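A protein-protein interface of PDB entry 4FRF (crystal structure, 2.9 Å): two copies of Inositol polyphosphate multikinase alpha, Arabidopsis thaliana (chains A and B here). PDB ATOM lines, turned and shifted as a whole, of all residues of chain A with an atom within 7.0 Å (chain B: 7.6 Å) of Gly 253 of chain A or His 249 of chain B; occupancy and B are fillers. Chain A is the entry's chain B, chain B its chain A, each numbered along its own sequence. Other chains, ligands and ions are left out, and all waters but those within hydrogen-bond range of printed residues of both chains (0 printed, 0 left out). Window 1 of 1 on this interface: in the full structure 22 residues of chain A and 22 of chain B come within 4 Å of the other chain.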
ATOM      1  N   GLY A  91     -13.810 -14.884  10.339  1.00  0.00           N
ATOM      2  CA  GLY A  91     -13.937 -16.312  10.510  1.00  0.00           C
ATOM      3  C   GLY A  91     -12.649 -17.047  10.298  1.00  0.00           C
ATOM      4  O   GLY A  91     -11.986 -16.868   9.277  1.00  0.00           O
ATOM      5  N   SER A  92     -12.305 -17.889  11.274  1.00  0.00           N
ATOM      6  CA  SER A  92     -11.081 -18.687  11.265  1.00  0.00           C
ATOM      7  C   SER A  92     -11.118 -19.695  10.117  1.00  0.00           C
ATOM      8  O   SER A  92     -10.089 -20.155   9.646  1.00  0.00           O
ATOM      9  CB  SER A  92     -10.936 -19.392  12.611  1.00  0.00           C
ATOM     10  OG  SER A  92      -9.712 -20.108  12.693  1.00  0.00           O
ATOM     11  N   THR A 115      -5.046 -14.420   5.012  1.00  0.00           N
ATOM     12  CA  THR A 115      -4.834 -14.270   6.432  1.00  0.00           C
ATOM     13  C   THR A 115      -5.991 -14.908   7.177  1.00  0.00           C
ATOM     14  O   THR A 115      -6.075 -14.812   8.395  1.00  0.00           O
ATOM     15  CB  THR A 115      -4.658 -12.795   6.839  1.00  0.00           C
ATOM     16  OG1 THR A 115      -5.872 -12.078   6.592  1.00  0.00           O
ATOM     17  CG2 THR A 115      -3.529 -12.159   6.042  1.00  0.00           C
ATOM     18  N   THR A 116      -6.867 -15.590   6.439  1.00  0.00           N
ATOM     19  CA  THR A 116      -8.056 -16.207   7.036  1.00  0.00           C
ATOM     20  C   THR A 116      -7.639 -17.311   7.957  1.00  0.00           C
ATOM     21  O   THR A 116      -8.173 -17.444   9.055  1.00  0.00           O
ATOM     22  CB  THR A 116      -9.001 -16.796   5.979  1.00  0.00           C
ATOM     23  OG1 THR A 116      -9.688 -15.732   5.299  1.00  0.00           O
ATOM     24  CG2 THR A 116     -10.026 -17.713   6.636  1.00  0.00           C
ATOM     25  N   VAL A 117      -6.693 -18.118   7.494  1.00  0.00           N
ATOM     26  CA  VAL A 117      -6.099 -19.156   8.319  1.00  0.00           C
ATOM     27  C   VAL A 117      -5.162 -18.551   9.350  1.00  0.00           C
ATOM     28  O   VAL A 117      -5.404 -18.663  10.549  1.00  0.00           O
ATOM     29  CB  VAL A 117      -5.320 -20.161   7.487  1.00  0.00           C
ATOM     30  CG1 VAL A 117      -4.900 -21.321   8.363  1.00  0.00           C
ATOM     31  CG2 VAL A 117      -6.158 -20.652   6.324  1.00  0.00           C
ATOM     32  N   SER A 118      -4.111 -17.887   8.877  1.00  0.00           N
ATOM     33  CA  SER A 118      -3.094 -17.321   9.762  1.00  0.00           C
ATOM     34  C   SER A 118      -3.657 -16.403  10.876  1.00  0.00           C
ATOM     35  O   SER A 118      -3.262 -16.491  12.039  1.00  0.00           O
ATOM     36  CB  SER A 118      -2.010 -16.605   8.949  1.00  0.00           C
ATOM     37  OG  SER A 118      -2.404 -15.289   8.598  1.00  0.00           O
ATOM     38  N   SER A 119      -4.586 -15.542  10.531  1.00  0.00           N
ATOM     39  CA  SER A 119      -5.234 -14.747  11.560  1.00  0.00           C
ATOM     40  C   SER A 119      -6.704 -15.077  11.550  1.00  0.00           C
ATOM     41  O   SER A 119      -7.142 -15.929  10.794  1.00  0.00           O
ATOM     42  CB  SER A 119      -5.001 -13.264  11.306  1.00  0.00           C
ATOM     43  OG  SER A 119      -3.743 -13.072  10.661  1.00  0.00           O
ATOM     44  N   GLY A 120      -7.482 -14.415  12.367  1.00  0.00           N
ATOM     45  CA  GLY A 120      -8.887 -14.780  12.432  1.00  0.00           C
ATOM     46  C   GLY A 120      -9.797 -14.248  11.321  1.00  0.00           C
ATOM     47  O   GLY A 120     -11.031 -14.316  11.442  1.00  0.00           O
ATOM     48  N   PHE A 121      -9.223 -13.703  10.253  1.00  0.00           N
ATOM     49  CA  PHE A 121     -10.005 -12.826   9.405  1.00  0.00           C
ATOM     50  C   PHE A 121      -9.305 -12.497   8.099  1.00  0.00           C
ATOM     51  O   PHE A 121      -8.185 -12.961   7.850  1.00  0.00           O
ATOM     52  CB  PHE A 121     -10.301 -11.542  10.159  1.00  0.00           C
ATOM     53  CG  PHE A 121      -9.071 -10.783  10.544  1.00  0.00           C
ATOM     54  CD1 PHE A 121      -8.571 -10.852  11.834  1.00  0.00           C
ATOM     55  CD2 PHE A 121      -8.387 -10.021   9.598  1.00  0.00           C
ATOM     56  CE1 PHE A 121      -7.410 -10.170  12.183  1.00  0.00           C
ATOM     57  CE2 PHE A 121      -7.228  -9.337   9.939  1.00  0.00           C
ATOM     58  CZ  PHE A 121      -6.741  -9.408  11.228  1.00  0.00           C
ATOM     59  N   ASP A 248     -20.730 -18.902  18.744  1.00  0.00           N
ATOM     60  CA  ASP A 248     -20.178 -18.816  17.394  1.00  0.00           C
ATOM     61  C   ASP A 248     -18.672 -18.684  17.506  1.00  0.00           C
ATOM     62  O   ASP A 248     -18.125 -17.603  17.403  1.00  0.00           O
ATOM     63  CB  ASP A 248     -20.777 -17.601  16.684  1.00  0.00           C
ATOM     64  CG  ASP A 248     -20.383 -17.513  15.231  1.00  0.00           C
ATOM     65  OD1 ASP A 248     -19.563 -18.317  14.740  1.00  0.00           O
ATOM     66  OD2 ASP A 248     -20.888 -16.608  14.575  1.00  0.00           O
ATOM     67  N   HIS A 249     -18.012 -19.770  17.847  1.00  0.00           N
ATOM     68  CA  HIS A 249     -16.630 -19.663  18.287  1.00  0.00           C
ATOM     69  C   HIS A 249     -15.756 -19.269  17.115  1.00  0.00           C
ATOM     70  O   HIS A 249     -14.819 -18.469  17.252  1.00  0.00           O
ATOM     71  CB  HIS A 249     -16.155 -20.964  18.917  1.00  0.00           C
ATOM     72  CG  HIS A 249     -16.431 -22.171  18.089  1.00  0.00           C
ATOM     73  ND1 HIS A 249     -15.596 -22.582  17.070  1.00  0.00           N
ATOM     74  CD2 HIS A 249     -17.423 -23.090  18.158  1.00  0.00           C
ATOM     75  CE1 HIS A 249     -16.060 -23.705  16.548  1.00  0.00           C
ATOM     76  NE2 HIS A 249     -17.169 -24.035  17.190  1.00  0.00           N
ATOM     77  N   ASN A 250     -16.135 -19.735  15.936  1.00  0.00           N
ATOM     78  CA  ASN A 250     -15.376 -19.422  14.764  1.00  0.00           C
ATOM     79  C   ASN A 250     -15.295 -17.903  14.516  1.00  0.00           C
ATOM     80  O   ASN A 250     -14.238 -17.374  14.170  1.00  0.00           O
ATOM     81  CB  ASN A 250     -15.948 -20.135  13.570  1.00  0.00           C
ATOM     82  CG  ASN A 250     -15.352 -19.666  12.302  1.00  0.00           C
ATOM     83  OD1 ASN A 250     -14.160 -19.834  12.067  1.00  0.00           O
ATOM     84  ND2 ASN A 250     -16.153 -19.015  11.487  1.00  0.00           N
ATOM     85  N   PHE A 251     -16.409 -17.212  14.723  1.00  0.00           N
ATOM     86  CA  PHE A 251     -16.424 -15.767  14.651  1.00  0.00           C
ATOM     87  C   PHE A 251     -15.652 -15.208  15.827  1.00  0.00           C
ATOM     88  O   PHE A 251     -14.750 -14.390  15.655  1.00  0.00           O
ATOM     89  CB  PHE A 251     -17.855 -15.253  14.693  1.00  0.00           C
ATOM     90  CG  PHE A 251     -18.016 -13.837  14.187  1.00  0.00           C
ATOM     91  CD1 PHE A 251     -18.368 -13.595  12.860  1.00  0.00           C
ATOM     92  CD2 PHE A 251     -17.912 -12.750  15.063  1.00  0.00           C
ATOM     93  CE1 PHE A 251     -18.548 -12.314  12.405  1.00  0.00           C
ATOM     94  CE2 PHE A 251     -18.122 -11.450  14.611  1.00  0.00           C
ATOM     95  CZ  PHE A 251     -18.425 -11.232  13.276  1.00  0.00           C
ATOM     96  N   LEU A 252     -15.990 -15.671  17.030  1.00  0.00           N
ATOM     97  CA  LEU A 252     -15.378 -15.132  18.247  1.00  0.00           C
ATOM     98  C   LEU A 252     -13.866 -15.236  18.173  1.00  0.00           C
ATOM     99  O   LEU A 252     -13.150 -14.333  18.610  1.00  0.00           O
ATOM    100  CB  LEU A 252     -15.887 -15.850  19.482  1.00  0.00           C
ATOM    101  CG  LEU A 252     -15.346 -15.241  20.771  1.00  0.00           C
ATOM    102  CD1 LEU A 252     -15.499 -13.731  20.759  1.00  0.00           C
ATOM    103  CD2 LEU A 252     -16.037 -15.822  21.980  1.00  0.00           C
ATOM    104  N   GLY A 253     -13.385 -16.321  17.578  1.00  0.00           N
ATOM    105  CA  GLY A 253     -11.969 -16.474  17.336  1.00  0.00           C
ATOM    106  C   GLY A 253     -11.468 -15.280  16.578  1.00  0.00           C
ATOM    107  O   GLY A 253     -10.745 -14.446  17.116  1.00  0.00           O
ATOM    108  N   GLY A 254     -11.960 -15.137  15.355  1.00  0.00           N
ATOM    109  CA  GLY A 254     -11.508 -14.079  14.450  1.00  0.00           C
ATOM    110  C   GLY A 254     -11.683 -12.691  15.029  1.00  0.00           C
ATOM    111  O   GLY A 254     -10.814 -11.839  14.880  1.00  0.00           O
ATOM    112  N   LEU A 255     -12.802 -12.462  15.707  1.00  0.00           N
ATOM    113  CA  LEU A 255     -13.090 -11.143  16.237  1.00  0.00           C
ATOM    114  C   LEU A 255     -11.956 -10.738  17.158  1.00  0.00           C
ATOM    115  O   LEU A 255     -11.404  -9.647  17.039  1.00  0.00           O
ATOM    116  CB  LEU A 255     -14.432 -11.137  16.993  1.00  0.00           C
ATOM    117  CG  LEU A 255     -14.887  -9.804  17.583  1.00  0.00           C
ATOM    118  CD1 LEU A 255     -14.818  -8.734  16.539  1.00  0.00           C
ATOM    119  CD2 LEU A 255     -16.278  -9.891  18.174  1.00  0.00           C
ATOM    120  N   CYS A 256     -11.543 -11.678  18.001  1.00  0.00           N
ATOM    121  CA  CYS A 256     -10.533 -11.423  19.013  1.00  0.00           C
ATOM    122  C   CYS A 256      -9.189 -11.129  18.380  1.00  0.00           C
ATOM    123  O   CYS A 256      -8.506 -10.183  18.779  1.00  0.00           O
ATOM    124  CB  CYS A 256     -10.437 -12.600  19.972  1.00  0.00           C
ATOM    125  SG  CYS A 256     -11.851 -12.725  21.074  1.00  0.00           S
ATOM    126  N   SER A 257      -8.818 -11.923  17.380  1.00  0.00           N
ATOM    127  CA  SER A 257      -7.617 -11.658  16.634  1.00  0.00           C
ATOM    128  C   SER A 257      -7.685 -10.234  16.102  1.00  0.00           C
ATOM    129  O   SER A 257      -6.788  -9.421  16.340  1.00  0.00           O
ATOM    130  CB  SER A 257      -7.489 -12.630  15.477  1.00  0.00           C
ATOM    131  OG  SER A 257      -6.202 -12.554  14.905  1.00  0.00           O
ATOM    132  N   PHE A 258      -8.779  -9.916  15.418  1.00  0.00           N
ATOM    133  CA  PHE A 258      -8.931  -8.609  14.813  1.00  0.00           C
ATOM    134  C   PHE A 258      -8.790  -7.554  15.883  1.00  0.00           C
ATOM    135  O   PHE A 258      -8.077  -6.582  15.713  1.00  0.00           O
ATOM    136  CB  PHE A 258     -10.290  -8.487  14.134  1.00  0.00           C
ATOM    137  CG  PHE A 258     -10.391  -7.332  13.186  1.00  0.00           C
ATOM    138  CD1 PHE A 258      -9.806  -7.402  11.912  1.00  0.00           C
ATOM    139  CD2 PHE A 258     -11.104  -6.192  13.535  1.00  0.00           C
ATOM    140  CE1 PHE A 258      -9.912  -6.337  11.014  1.00  0.00           C
ATOM    141  CE2 PHE A 258     -11.210  -5.129  12.648  1.00  0.00           C
ATOM    142  CZ  PHE A 258     -10.602  -5.202  11.382  1.00  0.00           C
ATOM    143  N   ILE A 259      -9.422  -7.779  17.015  1.00  0.00           N
ATOM    144  CA  ILE A 259      -9.347  -6.810  18.084  1.00  0.00           C
ATOM    145  C   ILE A 259      -7.891  -6.536  18.456  1.00  0.00           C
ATOM    146  O   ILE A 259      -7.480  -5.380  18.551  1.00  0.00           O
ATOM    147  CB  ILE A 259     -10.163  -7.247  19.302  1.00  0.00           C
ATOM    148  CG1 ILE A 259     -11.659  -7.238  18.938  1.00  0.00           C
ATOM    149  CG2 ILE A 259      -9.831  -6.361  20.497  1.00  0.00           C
ATOM    150  CD1 ILE A 259     -12.611  -7.313  20.103  1.00  0.00           C
ATOM    151  N   GLY B  91      -9.279 -26.701  20.338  1.00  0.00           N
ATOM    152  CA  GLY B  91      -9.062 -26.160  19.011  1.00  0.00           C
ATOM    153  C   GLY B  91     -10.204 -26.378  18.049  1.00  0.00           C
ATOM    154  O   GLY B  91     -10.615 -27.520  17.807  1.00  0.00           O
ATOM    155  N   SER B  92     -10.711 -25.261  17.504  1.00  0.00           N
ATOM    156  CA  SER B  92     -11.693 -25.248  16.412  1.00  0.00           C
ATOM    157  C   SER B  92     -11.243 -26.119  15.219  1.00  0.00           C
ATOM    158  O   SER B  92     -12.067 -26.671  14.496  1.00  0.00           O
ATOM    159  CB  SER B  92     -11.932 -23.802  15.968  1.00  0.00           C
ATOM    160  OG  SER B  92     -13.076 -23.679  15.130  1.00  0.00           O
ATOM    161  N   ARG B  93      -9.932 -26.209  15.019  1.00  0.00           N
ATOM    162  CA  ARG B  93      -9.333 -27.234  14.166  1.00  0.00           C
ATOM    163  C   ARG B  93      -8.137 -27.823  14.901  1.00  0.00           C
ATOM    164  O   ARG B  93      -7.651 -27.245  15.865  1.00  0.00           O
ATOM    165  CB  ARG B  93      -8.862 -26.633  12.847  1.00  0.00           C
ATOM    166  CG  ARG B  93      -7.833 -25.532  13.036  1.00  0.00           C
ATOM    167  CD  ARG B  93      -6.981 -25.314  11.805  1.00  0.00           C
ATOM    168  NE  ARG B  93      -5.882 -24.399  12.100  1.00  0.00           N
ATOM    169  CZ  ARG B  93      -5.982 -23.073  12.094  1.00  0.00           C
ATOM    170  NH1 ARG B  93      -7.130 -22.478  11.756  1.00  0.00           N
ATOM    171  NH2 ARG B  93      -4.926 -22.338  12.406  1.00  0.00           N
ATOM    172  N   PHE B 198      -5.229 -15.468  26.805  1.00  0.00           N
ATOM    173  CA  PHE B 198      -5.213 -15.843  25.394  1.00  0.00           C
ATOM    174  C   PHE B 198      -5.760 -14.745  24.485  1.00  0.00           C
ATOM    175  O   PHE B 198      -5.535 -14.754  23.273  1.00  0.00           O
ATOM    176  CB  PHE B 198      -5.971 -17.138  25.170  1.00  0.00           C
ATOM    177  CG  PHE B 198      -5.119 -18.345  25.249  1.00  0.00           C
ATOM    178  CD1 PHE B 198      -4.586 -18.904  24.100  1.00  0.00           C
ATOM    179  CD2 PHE B 198      -4.851 -18.940  26.468  1.00  0.00           C
ATOM    180  CE1 PHE B 198      -3.781 -20.035  24.169  1.00  0.00           C
ATOM    181  CE2 PHE B 198      -4.062 -20.067  26.545  1.00  0.00           C
ATOM    182  CZ  PHE B 198      -3.514 -20.612  25.396  1.00  0.00           C
ATOM    183  N   GLN B 201      -1.918 -12.591  24.659  1.00  0.00           N
ATOM    184  CA  GLN B 201      -0.598 -13.176  24.390  1.00  0.00           C
ATOM    185  C   GLN B 201      -0.416 -13.545  22.924  1.00  0.00           C
ATOM    186  O   GLN B 201      -1.268 -14.205  22.333  1.00  0.00           O
ATOM    187  CB  GLN B 201      -0.296 -14.384  25.319  1.00  0.00           C
ATOM    188  CG  GLN B 201      -0.855 -15.754  24.877  1.00  0.00           C
ATOM    189  CD  GLN B 201       0.006 -16.453  23.822  1.00  0.00           C
ATOM    190  OE1 GLN B 201       1.170 -16.098  23.605  1.00  0.00           O
ATOM    191  NE2 GLN B 201      -0.574 -17.438  23.150  1.00  0.00           N
ATOM    192  N   TYR B 204       3.133 -17.617  21.863  1.00  0.00           N
ATOM    193  CA  TYR B 204       3.080 -18.989  21.373  1.00  0.00           C
ATOM    194  C   TYR B 204       1.733 -19.282  20.724  1.00  0.00           C
ATOM    195  O   TYR B 204       0.704 -18.693  21.103  1.00  0.00           O
ATOM    196  CB  TYR B 204       3.351 -19.983  22.511  1.00  0.00           C
ATOM    197  CG  TYR B 204       4.627 -19.709  23.272  1.00  0.00           C
ATOM    198  CD1 TYR B 204       5.841 -20.223  22.836  1.00  0.00           C
ATOM    199  CD2 TYR B 204       4.623 -18.922  24.416  1.00  0.00           C
ATOM    200  CE1 TYR B 204       7.018 -19.962  23.516  1.00  0.00           C
ATOM    201  CE2 TYR B 204       5.795 -18.661  25.112  1.00  0.00           C
ATOM    202  CZ  TYR B 204       6.987 -19.180  24.656  1.00  0.00           C
ATOM    203  OH  TYR B 204       8.157 -18.916  25.333  1.00  0.00           O
ATOM    204  N   HIS B 205       1.770 -20.127  19.690  1.00  0.00           N
ATOM    205  CA  HIS B 205       0.572 -20.762  19.153  1.00  0.00           C
ATOM    206  C   HIS B 205       0.561 -22.216  19.586  1.00  0.00           C
ATOM    207  O   HIS B 205       1.435 -23.013  19.183  1.00  0.00           O
ATOM    208  CB  HIS B 205       0.553 -20.694  17.634  1.00  0.00           C
ATOM    209  CG  HIS B 205       0.211 -19.345  17.097  1.00  0.00           C
ATOM    210  ND1 HIS B 205       0.476 -18.975  15.794  1.00  0.00           N
ATOM    211  CD2 HIS B 205      -0.378 -18.274  17.683  1.00  0.00           C
ATOM    212  CE1 HIS B 205       0.067 -17.733  15.603  1.00  0.00           C
ATOM    213  NE2 HIS B 205      -0.459 -17.287  16.731  1.00  0.00           N
ATOM    214  N   VAL B 246       0.587 -12.783  16.548  1.00  0.00           N
ATOM    215  CA  VAL B 246      -0.800 -13.101  16.245  1.00  0.00           C
ATOM    216  C   VAL B 246      -1.331 -13.974  17.376  1.00  0.00           C
ATOM    217  O   VAL B 246      -0.748 -15.009  17.676  1.00  0.00           O
ATOM    218  CB  VAL B 246      -0.903 -13.888  14.916  1.00  0.00           C
ATOM    219  CG1 VAL B 246      -2.348 -14.224  14.598  1.00  0.00           C
ATOM    220  CG2 VAL B 246      -0.276 -13.112  13.790  1.00  0.00           C
ATOM    221  N   ILE B 247      -2.421 -13.562  18.018  1.00  0.00           N
ATOM    222  CA  ILE B 247      -2.962 -14.344  19.127  1.00  0.00           C
ATOM    223  C   ILE B 247      -3.249 -15.782  18.692  1.00  0.00           C
ATOM    224  O   ILE B 247      -3.272 -16.077  17.496  1.00  0.00           O
ATOM    225  CB  ILE B 247      -4.248 -13.727  19.732  1.00  0.00           C
ATOM    226  CG1 ILE B 247      -5.432 -13.857  18.776  1.00  0.00           C
ATOM    227  CG2 ILE B 247      -4.013 -12.293  20.250  1.00  0.00           C
ATOM    228  CD1 ILE B 247      -6.769 -13.564  19.456  1.00  0.00           C
ATOM    229  N   ASP B 248      -3.426 -16.686  19.664  1.00  0.00           N
ATOM    230  CA  ASP B 248      -3.824 -18.062  19.342  1.00  0.00           C
ATOM    231  C   ASP B 248      -5.341 -18.156  19.236  1.00  0.00           C
ATOM    232  O   ASP B 248      -6.009 -18.682  20.129  1.00  0.00           O
ATOM    233  CB  ASP B 248      -3.308 -19.051  20.380  1.00  0.00           C
ATOM    234  CG  ASP B 248      -3.348 -20.478  19.876  1.00  0.00           C
ATOM    235  OD1 ASP B 248      -4.037 -20.708  18.861  1.00  0.00           O
ATOM    236  OD2 ASP B 248      -2.667 -21.357  20.451  1.00  0.00           O
ATOM    237  N   HIS B 249      -5.885 -17.578  18.155  1.00  0.00           N
ATOM    238  CA  HIS B 249      -7.345 -17.426  17.990  1.00  0.00           C
ATOM    239  C   HIS B 249      -8.039 -18.795  17.941  1.00  0.00           C
ATOM    240  O   HIS B 249      -9.043 -19.031  18.642  1.00  0.00           O
ATOM    241  CB  HIS B 249      -7.681 -16.578  16.759  1.00  0.00           C
ATOM    242  CG  HIS B 249      -7.017 -17.041  15.498  1.00  0.00           C
ATOM    243  ND1 HIS B 249      -7.535 -18.046  14.711  1.00  0.00           N
ATOM    244  CD2 HIS B 249      -5.932 -16.569  14.834  1.00  0.00           C
ATOM    245  CE1 HIS B 249      -6.767 -18.211  13.643  1.00  0.00           C
ATOM    246  NE2 HIS B 249      -5.792 -17.322  13.689  1.00  0.00           N
ATOM    247  N   ASN B 250      -7.410 -19.732  17.242  1.00  0.00           N
ATOM    248  CA  ASN B 250      -7.893 -21.091  17.216  1.00  0.00           C
ATOM    249  C   ASN B 250      -8.119 -21.677  18.618  1.00  0.00           C
ATOM    250  O   ASN B 250      -9.216 -22.125  18.944  1.00  0.00           O
ATOM    251  CB  ASN B 250      -6.946 -21.954  16.433  1.00  0.00           C
ATOM    252  CG  ASN B 250      -7.154 -23.398  16.695  1.00  0.00           C
ATOM    253  OD1 ASN B 250      -8.138 -23.984  16.257  1.00  0.00           O
ATOM    254  ND2 ASN B 250      -6.224 -24.000  17.409  1.00  0.00           N
ATOM    255  N   PHE B 251      -7.096 -21.626  19.454  1.00  0.00           N
ATOM    256  CA  PHE B 251      -7.248 -21.992  20.855  1.00  0.00           C
ATOM    257  C   PHE B 251      -8.311 -21.137  21.556  1.00  0.00           C
ATOM    258  O   PHE B 251      -9.152 -21.660  22.276  1.00  0.00           O
ATOM    259  CB  PHE B 251      -5.915 -21.862  21.588  1.00  0.00           C
ATOM    260  CG  PHE B 251      -5.846 -22.643  22.868  1.00  0.00           C
ATOM    261  CD1 PHE B 251      -5.404 -23.966  22.871  1.00  0.00           C
ATOM    262  CD2 PHE B 251      -6.165 -22.050  24.077  1.00  0.00           C
ATOM    263  CE1 PHE B 251      -5.313 -24.663  24.034  1.00  0.00           C
ATOM    264  CE2 PHE B 251      -6.056 -22.756  25.257  1.00  0.00           C
ATOM    265  CZ  PHE B 251      -5.639 -24.061  25.234  1.00  0.00           C
ATOM    266  N   LEU B 252      -8.264 -19.822  21.357  1.00  0.00           N
ATOM    267  CA  LEU B 252      -9.114 -18.914  22.141  1.00  0.00           C
ATOM    268  C   LEU B 252     -10.575 -19.213  21.868  1.00  0.00           C
ATOM    269  O   LEU B 252     -11.426 -19.146  22.774  1.00  0.00           O
ATOM    270  CB  LEU B 252      -8.807 -17.451  21.812  1.00  0.00           C
ATOM    271  CG  LEU B 252      -9.694 -16.430  22.534  1.00  0.00           C
ATOM    272  CD1 LEU B 252      -9.623 -16.634  24.041  1.00  0.00           C
ATOM    273  CD2 LEU B 252      -9.325 -14.988  22.156  1.00  0.00           C
ATOM    274  N   GLY B 253     -10.859 -19.543  20.605  1.00  0.00           N
ATOM    275  CA  GLY B 253     -12.200 -19.912  20.198  1.00  0.00           C
ATOM    276  C   GLY B 253     -12.659 -21.118  20.983  1.00  0.00           C
ATOM    277  O   GLY B 253     -13.627 -21.049  21.753  1.00  0.00           O
ATOM    278  N   GLY B 254     -11.909 -22.208  20.838  1.00  0.00           N
ATOM    279  CA  GLY B 254     -12.158 -23.433  21.605  1.00  0.00           C
ATOM    280  C   GLY B 254     -12.395 -23.167  23.074  1.00  0.00           C
ATOM    281  O   GLY B 254     -13.421 -23.555  23.624  1.00  0.00           O
ATOM    282  N   LEU B 255     -11.469 -22.452  23.698  1.00  0.00           N
ATOM    283  CA  LEU B 255     -11.532 -22.219  25.120  1.00  0.00           C
ATOM    284  C   LEU B 255     -12.838 -21.531  25.461  1.00  0.00           C
ATOM    285  O   LEU B 255     -13.462 -21.824  26.475  1.00  0.00           O
ATOM    286  CB  LEU B 255     -10.346 -21.371  25.570  1.00  0.00           C
ATOM    287  CG  LEU B 255     -10.255 -21.092  27.066  1.00  0.00           C
ATOM    288  CD1 LEU B 255     -10.036 -22.396  27.823  1.00  0.00           C
ATOM    289  CD2 LEU B 255      -9.154 -20.074  27.395  1.00  0.00           C
ATOM    290  N   CYS B 256     -13.290 -20.657  24.577  1.00  0.00           N
ATOM    291  CA  CYS B 256     -14.478 -19.864  24.871  1.00  0.00           C
ATOM    292  C   CYS B 256     -15.750 -20.712  24.812  1.00  0.00           C
ATOM    293  O   CYS B 256     -16.597 -20.626  25.701  1.00  0.00           O
ATOM    294  CB  CYS B 256     -14.565 -18.631  23.960  1.00  0.00           C
ATOM    295  SG  CYS B 256     -13.461 -17.277  24.475  1.00  0.00           S
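Among the printed residues, pairs that only touch across the chains: Ser 92 of chain A with Arg 93 of chain B, Ser 92 of chain A with His 249 of chain B, Ser 118 of chain A with Val 246 of chain B, Gly 120 of chain A with His 249 of chain B, His 249 of chain A with Gly 253 of chain B, Leu 252 of chain A with Cys 256 of chain B, Gly 253 of chain A with His 249 of chain B, Cys 256 of chain A with Ile 247 of chain B, Cys 256 of chain A with Leu 252 of chain B and Ser 257 of chain A with Ile 247 of chain B.
OG of Ser 92 of chain B lies close to ND1 of His 249 of chain A. NE2 of His 249 of chain B sits close to O of Val 117 of chain A, at 3.4 Å. A ring nitrogen (NE2) of His 249 of chain B lies within hydrogen-bond range of the backbone carbonyl oxygen of Ser 118 of chain A (3.1 Å). O of Ser 119 of chain A sits close to NE2 of His 249 of chain B, at 3.5 Å.
N of Ser 92 of chain B lies within hydrogen-bond range of OD1 of Asn 250 of chain B, at 3.1 Å. The backbone NH (N) of Arg 93 of chain B sits at hydrogen-bond distance from the side-chain amide oxygen (OD1) of Asn 250 of chain B, 3.1 Å away. O of Val 246 of chain B is in hydrogen-bond range of NE2 of His 205 of chain B (2.5 Å). The side-chain hydroxyl (OG) of Ser 118 of chain A is in hydrogen-bond range of the side-chain hydroxyl (OG) of Ser 119 of chain A, 3.3 Å away. N of Gly 120 of chain A is in hydrogen-bond range of OG of Ser 257 of chain A, 3.4 Å away. The backbone carbonyl oxygen (O) of Leu 252 of chain A is in hydrogen-bond range of the side-chain sulfur (SG) of Cys 256 of chain A (3.2 Å).
Printed residues of chain A that touch a printed residue of chain B: Ser 92, Val 117, Ser 118, Ser 119, Gly 120, His 249, Leu 252, Gly 253, Cys 256 and Ser 257. Hydrophobic or aromatic side chains of chain A that line the printed part of chain B: His 249 and Leu 252. Of the 18 printed residues of chain B, 8 touch a printed residue of chain A. Hydrophobic or aromatic side chains of chain B that line the printed part of chain A: Val 246, Ile 247, His 249 and Leu 252. Among the printed residues, no Asp or Glu carboxylate lies within 4 Å of a Lys or Arg side-chain nitrogen of the other chain.
Printed residues of chain B within 4 Å of Ser 92 of chain A: Arg 93 and His 249. Of the printed residues of chain B, Gly 120 of chain A touches His 249 (3.6 Å). Of the printed residues of chain B, Leu 252 of chain A touches Cys 256 (3.7 Å). Gly 253 of chain A touches just one residue of chain B: His 249. Leu 255 of chain A touches none of the printed residues of chain B. Printed residues of chain A within 4 Å of Val 246 of chain B: Ser 118. His 249 of chain B touches six residues of chain A. Leu 255 of chain B touches none of the printed residues of chain A. The nearest residue of chain A that does not touch His 249 of chain B is Ser 257 of chain A (4.02 Å).
Ser 92 of chain A touches His 249 of chain B, and with the chains exchanged His 249 of chain A touches Ser 92 of chain B. His 249 of chain A touches Gly 253 of chain B, and with the chains exchanged Gly 253 of chain A touches His 249 of chain B. Leu 252 of chain A touches Cys 256 of chain B, and with the chains exchanged Cys 256 of chain A touches Leu 252 of chain B. 11 positions are printed for both chains.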
